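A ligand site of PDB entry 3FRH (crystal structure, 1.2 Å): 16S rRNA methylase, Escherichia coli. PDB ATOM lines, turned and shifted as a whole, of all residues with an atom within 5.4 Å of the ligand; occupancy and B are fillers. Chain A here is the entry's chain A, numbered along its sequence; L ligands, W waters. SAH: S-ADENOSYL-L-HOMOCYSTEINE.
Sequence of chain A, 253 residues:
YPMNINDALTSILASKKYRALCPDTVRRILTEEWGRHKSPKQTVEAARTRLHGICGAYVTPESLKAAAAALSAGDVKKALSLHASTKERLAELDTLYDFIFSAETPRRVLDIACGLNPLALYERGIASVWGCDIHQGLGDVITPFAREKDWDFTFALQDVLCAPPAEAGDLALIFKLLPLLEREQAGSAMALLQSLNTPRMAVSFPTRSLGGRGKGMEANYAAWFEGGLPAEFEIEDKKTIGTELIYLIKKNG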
ATOM      1  N   ARG A  28      13.360  14.273 -13.553  1.00  0.00           N
ATOM      2  CA  ARG A  28      12.817  14.405 -14.898  1.00  0.00           C
ATOM      3  C   ARG A  28      12.151  13.125 -15.360  1.00  0.00           C
ATOM      4  O   ARG A  28      11.006  13.133 -15.833  1.00  0.00           O
ATOM      5  CB  ARG A  28      13.918  14.813 -15.892  1.00  0.00           C
ATOM      6  CG  ARG A  28      13.455  14.854 -17.335  1.00  0.00           C
ATOM      7  CD  ARG A  28      14.502  15.376 -18.297  1.00  0.00           C
ATOM      8  NE  ARG A  28      15.744  14.596 -18.349  1.00  0.00           N
ATOM      9  CZ  ARG A  28      15.937  13.502 -19.080  1.00  0.00           C
ATOM     10  NH1 ARG A  28      14.951  12.997 -19.808  1.00  0.00           N
ATOM     11  NH2 ARG A  28      17.119  12.903 -19.055  1.00  0.00           N
ATOM     12  N   ILE A  54      19.943   5.031 -19.351  1.00  0.00           N
ATOM     13  CA  ILE A  54      20.669   6.280 -19.360  1.00  0.00           C
ATOM     14  C   ILE A  54      22.070   6.104 -18.774  1.00  0.00           C
ATOM     15  O   ILE A  54      23.054   6.611 -19.318  1.00  0.00           O
ATOM     16  CB  ILE A  54      19.862   7.384 -18.640  1.00  0.00           C
ATOM     17  CG1 ILE A  54      18.624   7.749 -19.481  1.00  0.00           C
ATOM     18  CG2 ILE A  54      20.713   8.599 -18.362  1.00  0.00           C
ATOM     19  CD1 ILE A  54      17.597   8.537 -18.720  1.00  0.00           C
ATOM     20  N   TYR A  58      28.603   2.395 -19.853  1.00  0.00           N
ATOM     21  CA  TYR A  58      29.845   3.133 -20.113  1.00  0.00           C
ATOM     22  C   TYR A  58      30.946   2.871 -19.092  1.00  0.00           C
ATOM     23  O   TYR A  58      32.119   2.730 -19.469  1.00  0.00           O
ATOM     24  CB  TYR A  58      29.590   4.640 -20.186  1.00  0.00           C
ATOM     25  CG  TYR A  58      28.419   5.059 -21.032  1.00  0.00           C
ATOM     26  CD1 TYR A  58      27.271   5.549 -20.437  1.00  0.00           C
ATOM     27  CD2 TYR A  58      28.447   4.972 -22.420  1.00  0.00           C
ATOM     28  CE1 TYR A  58      26.183   5.959 -21.175  1.00  0.00           C
ATOM     29  CE2 TYR A  58      27.350   5.363 -23.181  1.00  0.00           C
ATOM     30  CZ  TYR A  58      26.242   5.865 -22.538  1.00  0.00           C
ATOM     31  OH  TYR A  58      25.160   6.272 -23.288  1.00  0.00           O
ATOM     32  N   HIS A  83      36.353   4.204 -20.137  1.00  0.00           N
ATOM     33  CA  HIS A  83      34.979   4.625 -20.467  1.00  0.00           C
ATOM     34  C   HIS A  83      34.710   4.023 -21.831  1.00  0.00           C
ATOM     35  O   HIS A  83      35.540   4.188 -22.748  1.00  0.00           O
ATOM     36  CB  HIS A  83      34.860   6.135 -20.531  1.00  0.00           C
ATOM     37  CG  HIS A  83      33.462   6.625 -20.706  1.00  0.00           C
ATOM     38  ND1 HIS A  83      32.789   6.540 -21.911  1.00  0.00           N
ATOM     39  CD2 HIS A  83      32.613   7.214 -19.837  1.00  0.00           C
ATOM     40  CE1 HIS A  83      31.578   7.069 -21.761  1.00  0.00           C
ATOM     41  NE2 HIS A  83      31.448   7.474 -20.508  1.00  0.00           N
ATOM     42  N   SER A  85      32.982   4.796 -24.395  1.00  0.00           N
ATOM     43  CA  SER A  85      32.962   5.672 -25.577  1.00  0.00           C
ATOM     44  C   SER A  85      34.354   6.149 -25.978  1.00  0.00           C
ATOM     45  O   SER A  85      34.655   6.220 -27.168  1.00  0.00           O
ATOM     46  CB  SER A  85      32.065   6.884 -25.326  1.00  0.00           C
ATOM     47  OG  SER A  85      32.211   7.797 -26.396  1.00  0.00           O
ATOM     48  N   THR A  86      35.195   6.485 -25.008  1.00  0.00           N
ATOM     49  CA  THR A  86      36.576   6.851 -25.296  1.00  0.00           C
ATOM     50  C   THR A  86      37.401   5.641 -25.696  1.00  0.00           C
ATOM     51  O   THR A  86      38.320   5.771 -26.519  1.00  0.00           O
ATOM     52  CB  THR A  86      37.246   7.650 -24.153  1.00  0.00           C
ATOM     53  OG1 THR A  86      36.909   7.091 -22.883  1.00  0.00           O
ATOM     54  CG2 THR A  86      36.735   9.019 -24.152  1.00  0.00           C
ATOM     55  N   ARG A  89      37.174   5.223 -29.265  1.00  0.00           N
ATOM     56  CA  ARG A  89      37.870   6.333 -29.932  1.00  0.00           C
ATOM     57  C   ARG A  89      39.395   6.155 -29.940  1.00  0.00           C
ATOM     58  O   ARG A  89      40.092   6.810 -30.704  1.00  0.00           O
ATOM     59  CB  ARG A  89      37.485   7.682 -29.265  1.00  0.00           C
ATOM     60  CG  ARG A  89      37.991   8.926 -29.972  1.00  0.00           C
ATOM     61  CD  ARG A  89      37.300  10.111 -29.395  1.00  0.00           C
ATOM     62  NE  ARG A  89      35.855  10.007 -29.596  1.00  0.00           N
ATOM     63  CZ  ARG A  89      34.945   9.995 -28.614  1.00  0.00           C
ATOM     64  NH1 ARG A  89      35.324  10.103 -27.348  1.00  0.00           N
ATOM     65  NH2 ARG A  89      33.661   9.862 -28.915  1.00  0.00           N
ATOM     66  N   ASP A 111      32.500  20.488 -23.650  1.00  0.00           N
ATOM     67  CA  ASP A 111      32.366  19.067 -23.993  1.00  0.00           C
ATOM     68  C   ASP A 111      31.035  18.618 -23.399  1.00  0.00           C
ATOM     69  O   ASP A 111      30.897  18.473 -22.182  1.00  0.00           O
ATOM     70  CB  ASP A 111      33.565  18.280 -23.424  1.00  0.00           C
ATOM     71  CG  ASP A 111      33.689  16.898 -24.007  1.00  0.00           C
ATOM     72  OD1 ASP A 111      32.784  16.447 -24.759  1.00  0.00           O
ATOM     73  OD2 ASP A 111      34.711  16.244 -23.706  1.00  0.00           O
ATOM     74  N   ILE A 112      30.035  18.483 -24.282  1.00  0.00           N
ATOM     75  CA  ILE A 112      28.659  18.299 -23.837  1.00  0.00           C
ATOM     76  C   ILE A 112      28.358  16.813 -23.694  1.00  0.00           C
ATOM     77  O   ILE A 112      28.487  16.073 -24.657  1.00  0.00           O
ATOM     78  CB  ILE A 112      27.666  18.958 -24.838  1.00  0.00           C
ATOM     79  CG1 ILE A 112      28.092  20.393 -25.182  1.00  0.00           C
ATOM     80  CG2 ILE A 112      26.253  18.876 -24.294  1.00  0.00           C
ATOM     81  CD1 ILE A 112      28.250  21.295 -23.976  1.00  0.00           C
ATOM     82  N   ALA A 113      27.957  16.381 -22.489  1.00  0.00           N
ATOM     83  CA  ALA A 113      27.836  14.934 -22.171  1.00  0.00           C
ATOM     84  C   ALA A 113      29.223  14.308 -22.314  1.00  0.00           C
ATOM     85  O   ALA A 113      29.449  13.394 -23.118  1.00  0.00           O
ATOM     86  CB  ALA A 113      26.792  14.234 -23.022  1.00  0.00           C
ATOM     87  N   CYS A 114      30.158  14.816 -21.522  1.00  0.00           N
ATOM     88  CA  CYS A 114      31.577  14.647 -21.803  1.00  0.00           C
ATOM     89  C   CYS A 114      32.153  13.257 -21.597  1.00  0.00           C
ATOM     90  O   CYS A 114      33.233  12.978 -22.119  1.00  0.00           O
ATOM     91  CB  CYS A 114      32.387  15.671 -20.975  1.00  0.00           C
ATOM     92  SG  CYS A 114      32.251  15.503 -19.184  1.00  0.00           S
ATOM     93  N   GLY A 115      31.522  12.427 -20.770  1.00  0.00           N
ATOM     94  CA  GLY A 115      32.166  11.163 -20.450  1.00  0.00           C
ATOM     95  C   GLY A 115      33.545  11.411 -19.842  1.00  0.00           C
ATOM     96  O   GLY A 115      33.721  12.304 -19.022  1.00  0.00           O
ATOM     97  N   LEU A 116      34.516  10.602 -20.261  1.00  0.00           N
ATOM     98  CA  LEU A 116      35.916  10.836 -19.881  1.00  0.00           C
ATOM     99  C   LEU A 116      36.718  11.527 -20.992  1.00  0.00           C
ATOM    100  O   LEU A 116      37.938  11.680 -20.881  1.00  0.00           O
ATOM    101  CB  LEU A 116      36.630   9.555 -19.442  1.00  0.00           C
ATOM    102  CG  LEU A 116      36.122   8.916 -18.145  1.00  0.00           C
ATOM    103  CD1 LEU A 116      37.000   7.733 -17.789  1.00  0.00           C
ATOM    104  CD2 LEU A 116      36.071   9.907 -16.984  1.00  0.00           C
ATOM    105  N   ASN A 117      36.044  11.952 -22.057  1.00  0.00           N
ATOM    106  CA  ASN A 117      36.728  12.584 -23.169  1.00  0.00           C
ATOM    107  C   ASN A 117      37.589  13.796 -22.787  1.00  0.00           C
ATOM    108  O   ASN A 117      38.581  14.042 -23.469  1.00  0.00           O
ATOM    109  CB  ASN A 117      35.729  12.919 -24.274  1.00  0.00           C
ATOM    110  CG  ASN A 117      36.398  13.558 -25.460  1.00  0.00           C
ATOM    111  OD1 ASN A 117      37.097  12.888 -26.235  1.00  0.00           O
ATOM    112  ND2 ASN A 117      36.209  14.855 -25.622  1.00  0.00           N
ATOM    113  N   CYS A 132      30.061  18.817 -19.162  1.00  0.00           N
ATOM    114  CA  CYS A 132      28.885  18.483 -18.377  1.00  0.00           C
ATOM    115  C   CYS A 132      28.460  17.052 -18.650  1.00  0.00           C
ATOM    116  O   CYS A 132      28.626  16.544 -19.753  1.00  0.00           O
ATOM    117  CB  CYS A 132      27.731  19.452 -18.625  1.00  0.00           C
ATOM    118  SG  CYS A 132      27.019  19.456 -20.293  1.00  0.00           S
ATOM    119  N   ASP A 133      27.888  16.425 -17.630  1.00  0.00           N
ATOM    120  CA  ASP A 133      27.335  15.094 -17.781  1.00  0.00           C
ATOM    121  C   ASP A 133      26.417  14.835 -16.591  1.00  0.00           C
ATOM    122  O   ASP A 133      26.274  15.676 -15.711  1.00  0.00           O
ATOM    123  CB  ASP A 133      28.464  14.036 -17.894  1.00  0.00           C
ATOM    124  CG  ASP A 133      28.066  12.812 -18.702  1.00  0.00           C
ATOM    125  OD1 ASP A 133      27.119  12.102 -18.256  1.00  0.00           O
ATOM    126  OD2 ASP A 133      28.693  12.554 -19.752  1.00  0.00           O
ATOM    127  N   ILE A 134      25.795  13.660 -16.567  1.00  0.00           N
ATOM    128  CA  ILE A 134      24.830  13.311 -15.538  1.00  0.00           C
ATOM    129  C   ILE A 134      25.343  12.261 -14.570  1.00  0.00           C
ATOM    130  O   ILE A 134      24.610  11.848 -13.678  1.00  0.00           O
ATOM    131  CB  ILE A 134      23.481  12.873 -16.162  1.00  0.00           C
ATOM    132  CG1 ILE A 134      23.688  11.751 -17.186  1.00  0.00           C
ATOM    133  CG2 ILE A 134      22.774  14.068 -16.785  1.00  0.00           C
ATOM    134  CD1 ILE A 134      22.446  11.143 -17.624  1.00  0.00           C
ATOM    135  N   HIS A 135      26.598  11.828 -14.715  1.00  0.00           N
ATOM    136  CA  HIS A 135      27.201  10.858 -13.806  1.00  0.00           C
ATOM    137  C   HIS A 135      28.326  11.554 -13.069  1.00  0.00           C
ATOM    138  O   HIS A 135      29.356  11.901 -13.669  1.00  0.00           O
ATOM    139  CB  HIS A 135      27.725   9.690 -14.615  1.00  0.00           C
ATOM    140  CG  HIS A 135      28.166   8.514 -13.795  1.00  0.00           C
ATOM    141  ND1 HIS A 135      28.748   8.647 -12.550  1.00  0.00           N
ATOM    142  CD2 HIS A 135      28.161   7.196 -14.078  1.00  0.00           C
ATOM    143  CE1 HIS A 135      29.035   7.440 -12.081  1.00  0.00           C
ATOM    144  NE2 HIS A 135      28.700   6.547 -12.995  1.00  0.00           N
ATOM    145  N   LEU A 138      32.197  10.716 -13.267  1.00  0.00           N
ATOM    146  CA  LEU A 138      33.087  11.229 -14.312  1.00  0.00           C
ATOM    147  C   LEU A 138      33.890  12.425 -13.808  1.00  0.00           C
ATOM    148  O   LEU A 138      35.116  12.475 -13.974  1.00  0.00           O
ATOM    149  CB  LEU A 138      32.265  11.639 -15.519  1.00  0.00           C
ATOM    150  CG  LEU A 138      31.411  10.522 -16.125  1.00  0.00           C
ATOM    151  CD1 LEU A 138      30.403  11.094 -17.110  1.00  0.00           C
ATOM    152  CD2 LEU A 138      32.282   9.435 -16.770  1.00  0.00           C
ATOM    153  N   GLN A 158      24.987  18.150 -14.894  1.00  0.00           N
ATOM    154  CA  GLN A 158      23.918  18.878 -15.554  1.00  0.00           C
ATOM    155  C   GLN A 158      23.293  18.025 -16.645  1.00  0.00           C
ATOM    156  O   GLN A 158      23.982  17.486 -17.508  1.00  0.00           O
ATOM    157  CB  GLN A 158      24.453  20.174 -16.163  1.00  0.00           C
ATOM    158  CG  GLN A 158      23.361  20.991 -16.858  1.00  0.00           C
ATOM    159  CD  GLN A 158      23.840  22.341 -17.355  1.00  0.00           C
ATOM    160  OE1 GLN A 158      24.867  22.844 -16.922  1.00  0.00           O
ATOM    161  NE2 GLN A 158      23.078  22.940 -18.284  1.00  0.00           N
ATOM    162  N   ASP A 159      21.969  17.896 -16.570  1.00  0.00           N
ATOM    163  CA  ASP A 159      21.172  17.220 -17.573  1.00  0.00           C
ATOM    164  C   ASP A 159      20.739  18.261 -18.596  1.00  0.00           C
ATOM    165  O   ASP A 159      20.020  19.217 -18.280  1.00  0.00           O
ATOM    166  CB  ASP A 159      19.954  16.597 -16.870  1.00  0.00           C
ATOM    167  CG  ASP A 159      19.095  15.763 -17.797  1.00  0.00           C
ATOM    168  OD1 ASP A 159      18.918  16.140 -18.979  1.00  0.00           O
ATOM    169  OD2 ASP A 159      18.583  14.715 -17.315  1.00  0.00           O
ATOM    170  N   VAL A 160      21.190  18.097 -19.845  1.00  0.00           N
ATOM    171  CA  VAL A 160      20.930  19.113 -20.858  1.00  0.00           C
ATOM    172  C   VAL A 160      19.472  19.162 -21.309  1.00  0.00           C
ATOM    173  O   VAL A 160      19.060  20.119 -21.959  1.00  0.00           O
ATOM    174  CB  VAL A 160      21.882  18.982 -22.065  1.00  0.00           C
ATOM    175  CG1 VAL A 160      23.332  19.104 -21.607  1.00  0.00           C
ATOM    176  CG2 VAL A 160      21.627  17.678 -22.838  1.00  0.00           C
ATOM    177  N   LEU A 161      18.677  18.160 -20.929  1.00  0.00           N
ATOM    178  CA  LEU A 161      17.234  18.213 -21.155  1.00  0.00           C
ATOM    179  C   LEU A 161      16.513  18.987 -20.055  1.00  0.00           C
ATOM    180  O   LEU A 161      15.345  19.362 -20.200  1.00  0.00           O
ATOM    181  CB  LEU A 161      16.633  16.818 -21.321  1.00  0.00           C
ATOM    182  CG  LEU A 161      17.167  16.034 -22.518  1.00  0.00           C
ATOM    183  CD1 LEU A 161      16.611  14.627 -22.538  1.00  0.00           C
ATOM    184  CD2 LEU A 161      16.870  16.763 -23.845  1.00  0.00           C
ATOM    185  N   PHE A 175      29.606  14.635 -28.922  1.00  0.00           N
ATOM    186  CA  PHE A 175      29.984  13.325 -29.425  1.00  0.00           C
ATOM    187  C   PHE A 175      29.061  12.233 -28.890  1.00  0.00           C
ATOM    188  O   PHE A 175      28.893  12.110 -27.669  1.00  0.00           O
ATOM    189  CB  PHE A 175      31.394  12.927 -29.010  1.00  0.00           C
ATOM    190  CG  PHE A 175      32.526  13.746 -29.605  1.00  0.00           C
ATOM    191  CD1 PHE A 175      33.813  13.532 -29.113  1.00  0.00           C
ATOM    192  CD2 PHE A 175      32.362  14.675 -30.636  1.00  0.00           C
ATOM    193  CE1 PHE A 175      34.898  14.209 -29.620  1.00  0.00           C
ATOM    194  CE2 PHE A 175      33.467  15.358 -31.151  1.00  0.00           C
ATOM    195  CZ  PHE A 175      34.737  15.121 -30.629  1.00  0.00           C
ATOM    196  N   LYS A 176      28.477  11.465 -29.797  1.00  0.00           N
ATOM    197  CA  LYS A 176      27.699  10.281 -29.426  1.00  0.00           C
ATOM    198  C   LYS A 176      26.545  10.605 -28.482  1.00  0.00           C
ATOM    199  O   LYS A 176      26.203   9.803 -27.602  1.00  0.00           O
ATOM    200  CB  LYS A 176      28.623   9.181 -28.851  1.00  0.00           C
ATOM    201  CG  LYS A 176      29.652   8.681 -29.858  1.00  0.00           C
ATOM    202  CD  LYS A 176      30.679   7.760 -29.223  1.00  0.00           C
ATOM    203  CE  LYS A 176      31.715   7.289 -30.218  1.00  0.00           C
ATOM    204  NZ  LYS A 176      32.748   6.413 -29.577  1.00  0.00           N
ATOM    205  N   LEU A 177      25.932  11.767 -28.686  1.00  0.00           N
ATOM    206  CA  LEU A 177      24.892  12.287 -27.787  1.00  0.00           C
ATOM    207  C   LEU A 177      23.571  12.562 -28.506  1.00  0.00           C
ATOM    208  O   LEU A 177      22.496  12.284 -27.963  1.00  0.00           O
ATOM    209  CB  LEU A 177      25.361  13.569 -27.089  1.00  0.00           C
ATOM    210  CG  LEU A 177      24.315  14.202 -26.175  1.00  0.00           C
ATOM    211  CD1 LEU A 177      23.947  13.285 -24.978  1.00  0.00           C
ATOM    212  CD2 LEU A 177      24.749  15.568 -25.703  1.00  0.00           C
ATOM    213  N   LEU A 180      20.776   9.751 -28.632  1.00  0.00           N
ATOM    214  CA  LEU A 180      20.088   9.360 -27.424  1.00  0.00           C
ATOM    215  C   LEU A 180      19.164  10.479 -26.935  1.00  0.00           C
ATOM    216  O   LEU A 180      18.107  10.209 -26.353  1.00  0.00           O
ATOM    217  CB  LEU A 180      21.066   8.877 -26.340  1.00  0.00           C
ATOM    218  CG  LEU A 180      21.893   9.914 -25.612  1.00  0.00           C
ATOM    219  CD1 LEU A 180      21.123  10.539 -24.448  1.00  0.00           C
ATOM    220  CD2 LEU A 180      23.185   9.277 -25.094  1.00  0.00           C
ATOM    221  N   LEU A 181      19.531  11.739 -27.180  1.00  0.00           N
ATOM    222  CA  LEU A 181      18.640  12.840 -26.800  1.00  0.00           C
ATOM    223  C   LEU A 181      17.368  12.811 -27.633  1.00  0.00           C
ATOM    224  O   LEU A 181      16.268  12.966 -27.095  1.00  0.00           O
ATOM    225  CB  LEU A 181      19.306  14.195 -26.997  1.00  0.00           C
ATOM    226  CG  LEU A 181      20.474  14.485 -26.057  1.00  0.00           C
ATOM    227  CD1 LEU A 181      21.026  15.856 -26.387  1.00  0.00           C
ATOM    228  CD2 LEU A 181      20.069  14.400 -24.566  1.00  0.00           C
ATOM    229  N   GLU A 184      14.793  10.215 -26.729  1.00  0.00           N
ATOM    230  CA  GLU A 184      14.150  10.524 -25.466  1.00  0.00           C
ATOM    231  C   GLU A 184      13.196  11.712 -25.513  1.00  0.00           C
ATOM    232  O   GLU A 184      12.223  11.775 -24.759  1.00  0.00           O
ATOM    233  CB  GLU A 184      15.217  10.780 -24.430  1.00  0.00           C
ATOM    234  CG  GLU A 184      14.704  10.613 -23.058  1.00  0.00           C
ATOM    235  CD  GLU A 184      15.817  10.464 -22.070  1.00  0.00           C
ATOM    236  OE1 GLU A 184      16.995  10.296 -22.477  1.00  0.00           O
ATOM    237  OE2 GLU A 184      15.523  10.516 -20.876  1.00  0.00           O
ATOM    238  N   GLU A 244      33.391   6.565 -35.964  1.00  0.00           N
ATOM    239  CA  GLU A 244      32.595   7.772 -35.776  1.00  0.00           C
ATOM    240  C   GLU A 244      32.475   8.546 -37.084  1.00  0.00           C
ATOM    241  O   GLU A 244      33.437   8.679 -37.847  1.00  0.00           O
ATOM    242  CB  GLU A 244      33.232   8.705 -34.741  1.00  0.00           C
ATOM    243  CG  GLU A 244      32.853   8.440 -33.294  1.00  0.00           C
ATOM    244  CD  GLU A 244      33.619   9.354 -32.337  1.00  0.00           C
ATOM    245  OE1 GLU A 244      32.991  10.207 -31.673  1.00  0.00           O
ATOM    246  OE2 GLU A 244      34.862   9.202 -32.239  1.00  0.00           O
HETATM  247  N   SAH L   1      30.721  12.439 -25.333  1.00  0.00           N
HETATM  248  CA  SAH L   1      31.427  11.333 -24.677  1.00  0.00           C
HETATM  249  CB  SAH L   1      30.469  10.340 -24.008  1.00  0.00           C
HETATM  250  CG  SAH L   1      29.469   9.735 -24.999  1.00  0.00           C
HETATM  251  SD  SAH L   1      28.392   8.495 -24.233  1.00  0.00           S
HETATM  252  C   SAH L   1      32.303  10.625 -25.687  1.00  0.00           C
HETATM  253  O   SAH L   1      31.966  10.663 -26.882  1.00  0.00           O
HETATM  254  OXT SAH L   1      33.312   9.995 -25.285  1.00  0.00           O
HETATM  255  C5' SAH L   1      26.897   9.464 -23.911  1.00  0.00           C
HETATM  256  C4' SAH L   1      27.022  10.358 -22.679  1.00  0.00           C
HETATM  257  O4' SAH L   1      25.805  11.096 -22.557  1.00  0.00           O
HETATM  258  C3' SAH L   1      27.206   9.599 -21.360  1.00  0.00           C
HETATM  259  O3' SAH L   1      28.364  10.033 -20.658  1.00  0.00           O
HETATM  260  C2' SAH L   1      25.912   9.904 -20.617  1.00  0.00           C
HETATM  261  O2' SAH L   1      25.999   9.902 -19.214  1.00  0.00           O
HETATM  262  C1' SAH L   1      25.538  11.264 -21.170  1.00  0.00           C
HETATM  263  N9  SAH L   1      24.138  11.682 -21.051  1.00  0.00           N
HETATM  264  C8  SAH L   1      23.020  10.935 -21.326  1.00  0.00           C
HETATM  265  N7  SAH L   1      21.923  11.691 -21.198  1.00  0.00           N
HETATM  266  C5  SAH L   1      22.337  12.939 -20.850  1.00  0.00           C
HETATM  267  C6  SAH L   1      21.644  14.119 -20.581  1.00  0.00           C
HETATM  268  N6  SAH L   1      20.302  14.195 -20.642  1.00  0.00           N
HETATM  269  N1  SAH L   1      22.364  15.227 -20.240  1.00  0.00           N
HETATM  270  C2  SAH L   1      23.735  15.153 -20.164  1.00  0.00           C
HETATM  271  N3  SAH L   1      24.455  14.030 -20.428  1.00  0.00           N
HETATM  272  C4  SAH L   1      23.733  12.947 -20.768  1.00  0.00           C
HETATM  273  O   HOH W   1      23.146   7.556 -21.879  1.00  0.00           O
HETATM  274  O   HOH W   2      33.850   9.238 -22.724  1.00  0.00           O
HETATM  275  O   HOH W   3      33.101  13.993 -25.788  1.00  0.00           O
HETATM  276  O   HOH W   4      19.065  11.346 -20.861  1.00  0.00           O
HETATM  277  O   HOH W   5      25.026   7.772 -17.845  1.00  0.00           O
HETATM  278  O   HOH W   6      26.518   7.113 -26.821  1.00  0.00           O
HETATM  279  O   HOH W   7      30.485  15.355 -26.329  1.00  0.00           O
HETATM  280  O   HOH W   8      29.331   8.212 -18.875  1.00  0.00           O
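Water W5 bridges O2' of the ligand and O of Ile 54.
Water W2 lies within hydrogen-bond range of OXT of the ligand, N of Leu 116 and ND1 of His 83.
Water W8 lies within hydrogen-bond range of an oxygen (O3') of the ligand (2.7 Å) and a ring nitrogen (NE2) of His 83 (2.8 Å).
Water W3 lies within hydrogen-bond range of the side-chain carboxylate (OD1) of Asp 111 (2.7 Å), a nitrogen (N) of the ligand (2.9 Å) and the side-chain amide nitrogen (ND2) of Asn 117 (3.2 Å).
Water W4 lies within hydrogen-bond range of the side-chain carboxylate of Glu 184 (2.8 Å), a nitrogen (N7) of the ligand (2.9 Å) and the guanidinium group of Arg 28 (3.1 Å).
Water W1 lies within hydrogen-bond range of O of Ile 54 (2.7 Å) and OH of Tyr 58 (2.8 Å).
Residues that only touch the ligand: Tyr 58 (3.5 Å), Cys 114 (3.5 Å), Leu 180 (3.5 Å), Gln 158 (3.5 Å), Ile 134 (3.6 Å), Thr 86 (3.7 Å), Leu 177 (3.8 Å), Lys 176 (3.8 Å), Arg 28 (3.8 Å), Asn 117 (3.9 Å), Leu 181 (3.9 Å) and Gly 115 (3.96 Å).
19 residues have an atom within 4 Å of the ligand: Arg 28, Tyr 58, Ser 85, Thr 86, Arg 89, Ala 113, Cys 114, Gly 115, Asn 117, Asp 133, Ile 134, Gln 158, Asp 159, Val 160, Phe 175, Lys 176, Leu 177, Leu 180 and Leu 181.
The backbone carbonyl oxygen of Cys 132 lies within hydrogen-bond range of the backbone NH of Ala 113 (2.8 Å).
OE2 of Glu 184 lies within salt-bridge range of NH1 of Arg 28, at 2.8 Å.
OD1 of Asn 117 sits at hydrogen-bond distance from NH1 of Arg 89.
The side-chain carboxylate (OD2) of Asp 133 sits at hydrogen-bond distance from the backbone NH (N) of Gly 115 (3.0 Å).
The side-chain hydroxyl (OG1) of Thr 86 sits at hydrogen-bond distance from the backbone carbonyl oxygen (O) of His 83 (3.2 Å).
The side-chain carboxylate (OD2) of Asp 133 sits at hydrogen-bond distance from the backbone NH (N) of Cys 114 (3.2 Å).
OD1 of Asp 159 lies within hydrogen-bond range of N of Leu 161 (2.8 Å).
N of Ser 85 is in hydrogen-bond range of ND1 of His 83 (3.0 Å).
The backbone carbonyl oxygen (O) of Phe 175 sits at hydrogen-bond distance from a nitrogen (N) of the ligand (3.0 Å).
N of Val 160 sits at hydrogen-bond distance from N1 of the ligand, at 3.1 Å.
N6 of the ligand is in hydrogen-bond range of OD1 of Asp 159, 2.9 Å away.
A nitrogen (N) of the ligand lies within hydrogen-bond range of the backbone carbonyl oxygen (O) of Ala 113 (2.7 Å).
An oxygen (OXT) of the ligand lies within hydrogen-bond range of the side-chain hydroxyl of Ser 85 (2.7 Å).
The side-chain carboxylate of Asp 133 lies within hydrogen-bond range of an oxygen (O2') of the ligand (2.6 Å).
O of the ligand is in salt-bridge range of NH2 of Arg 89 (2.8 Å).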
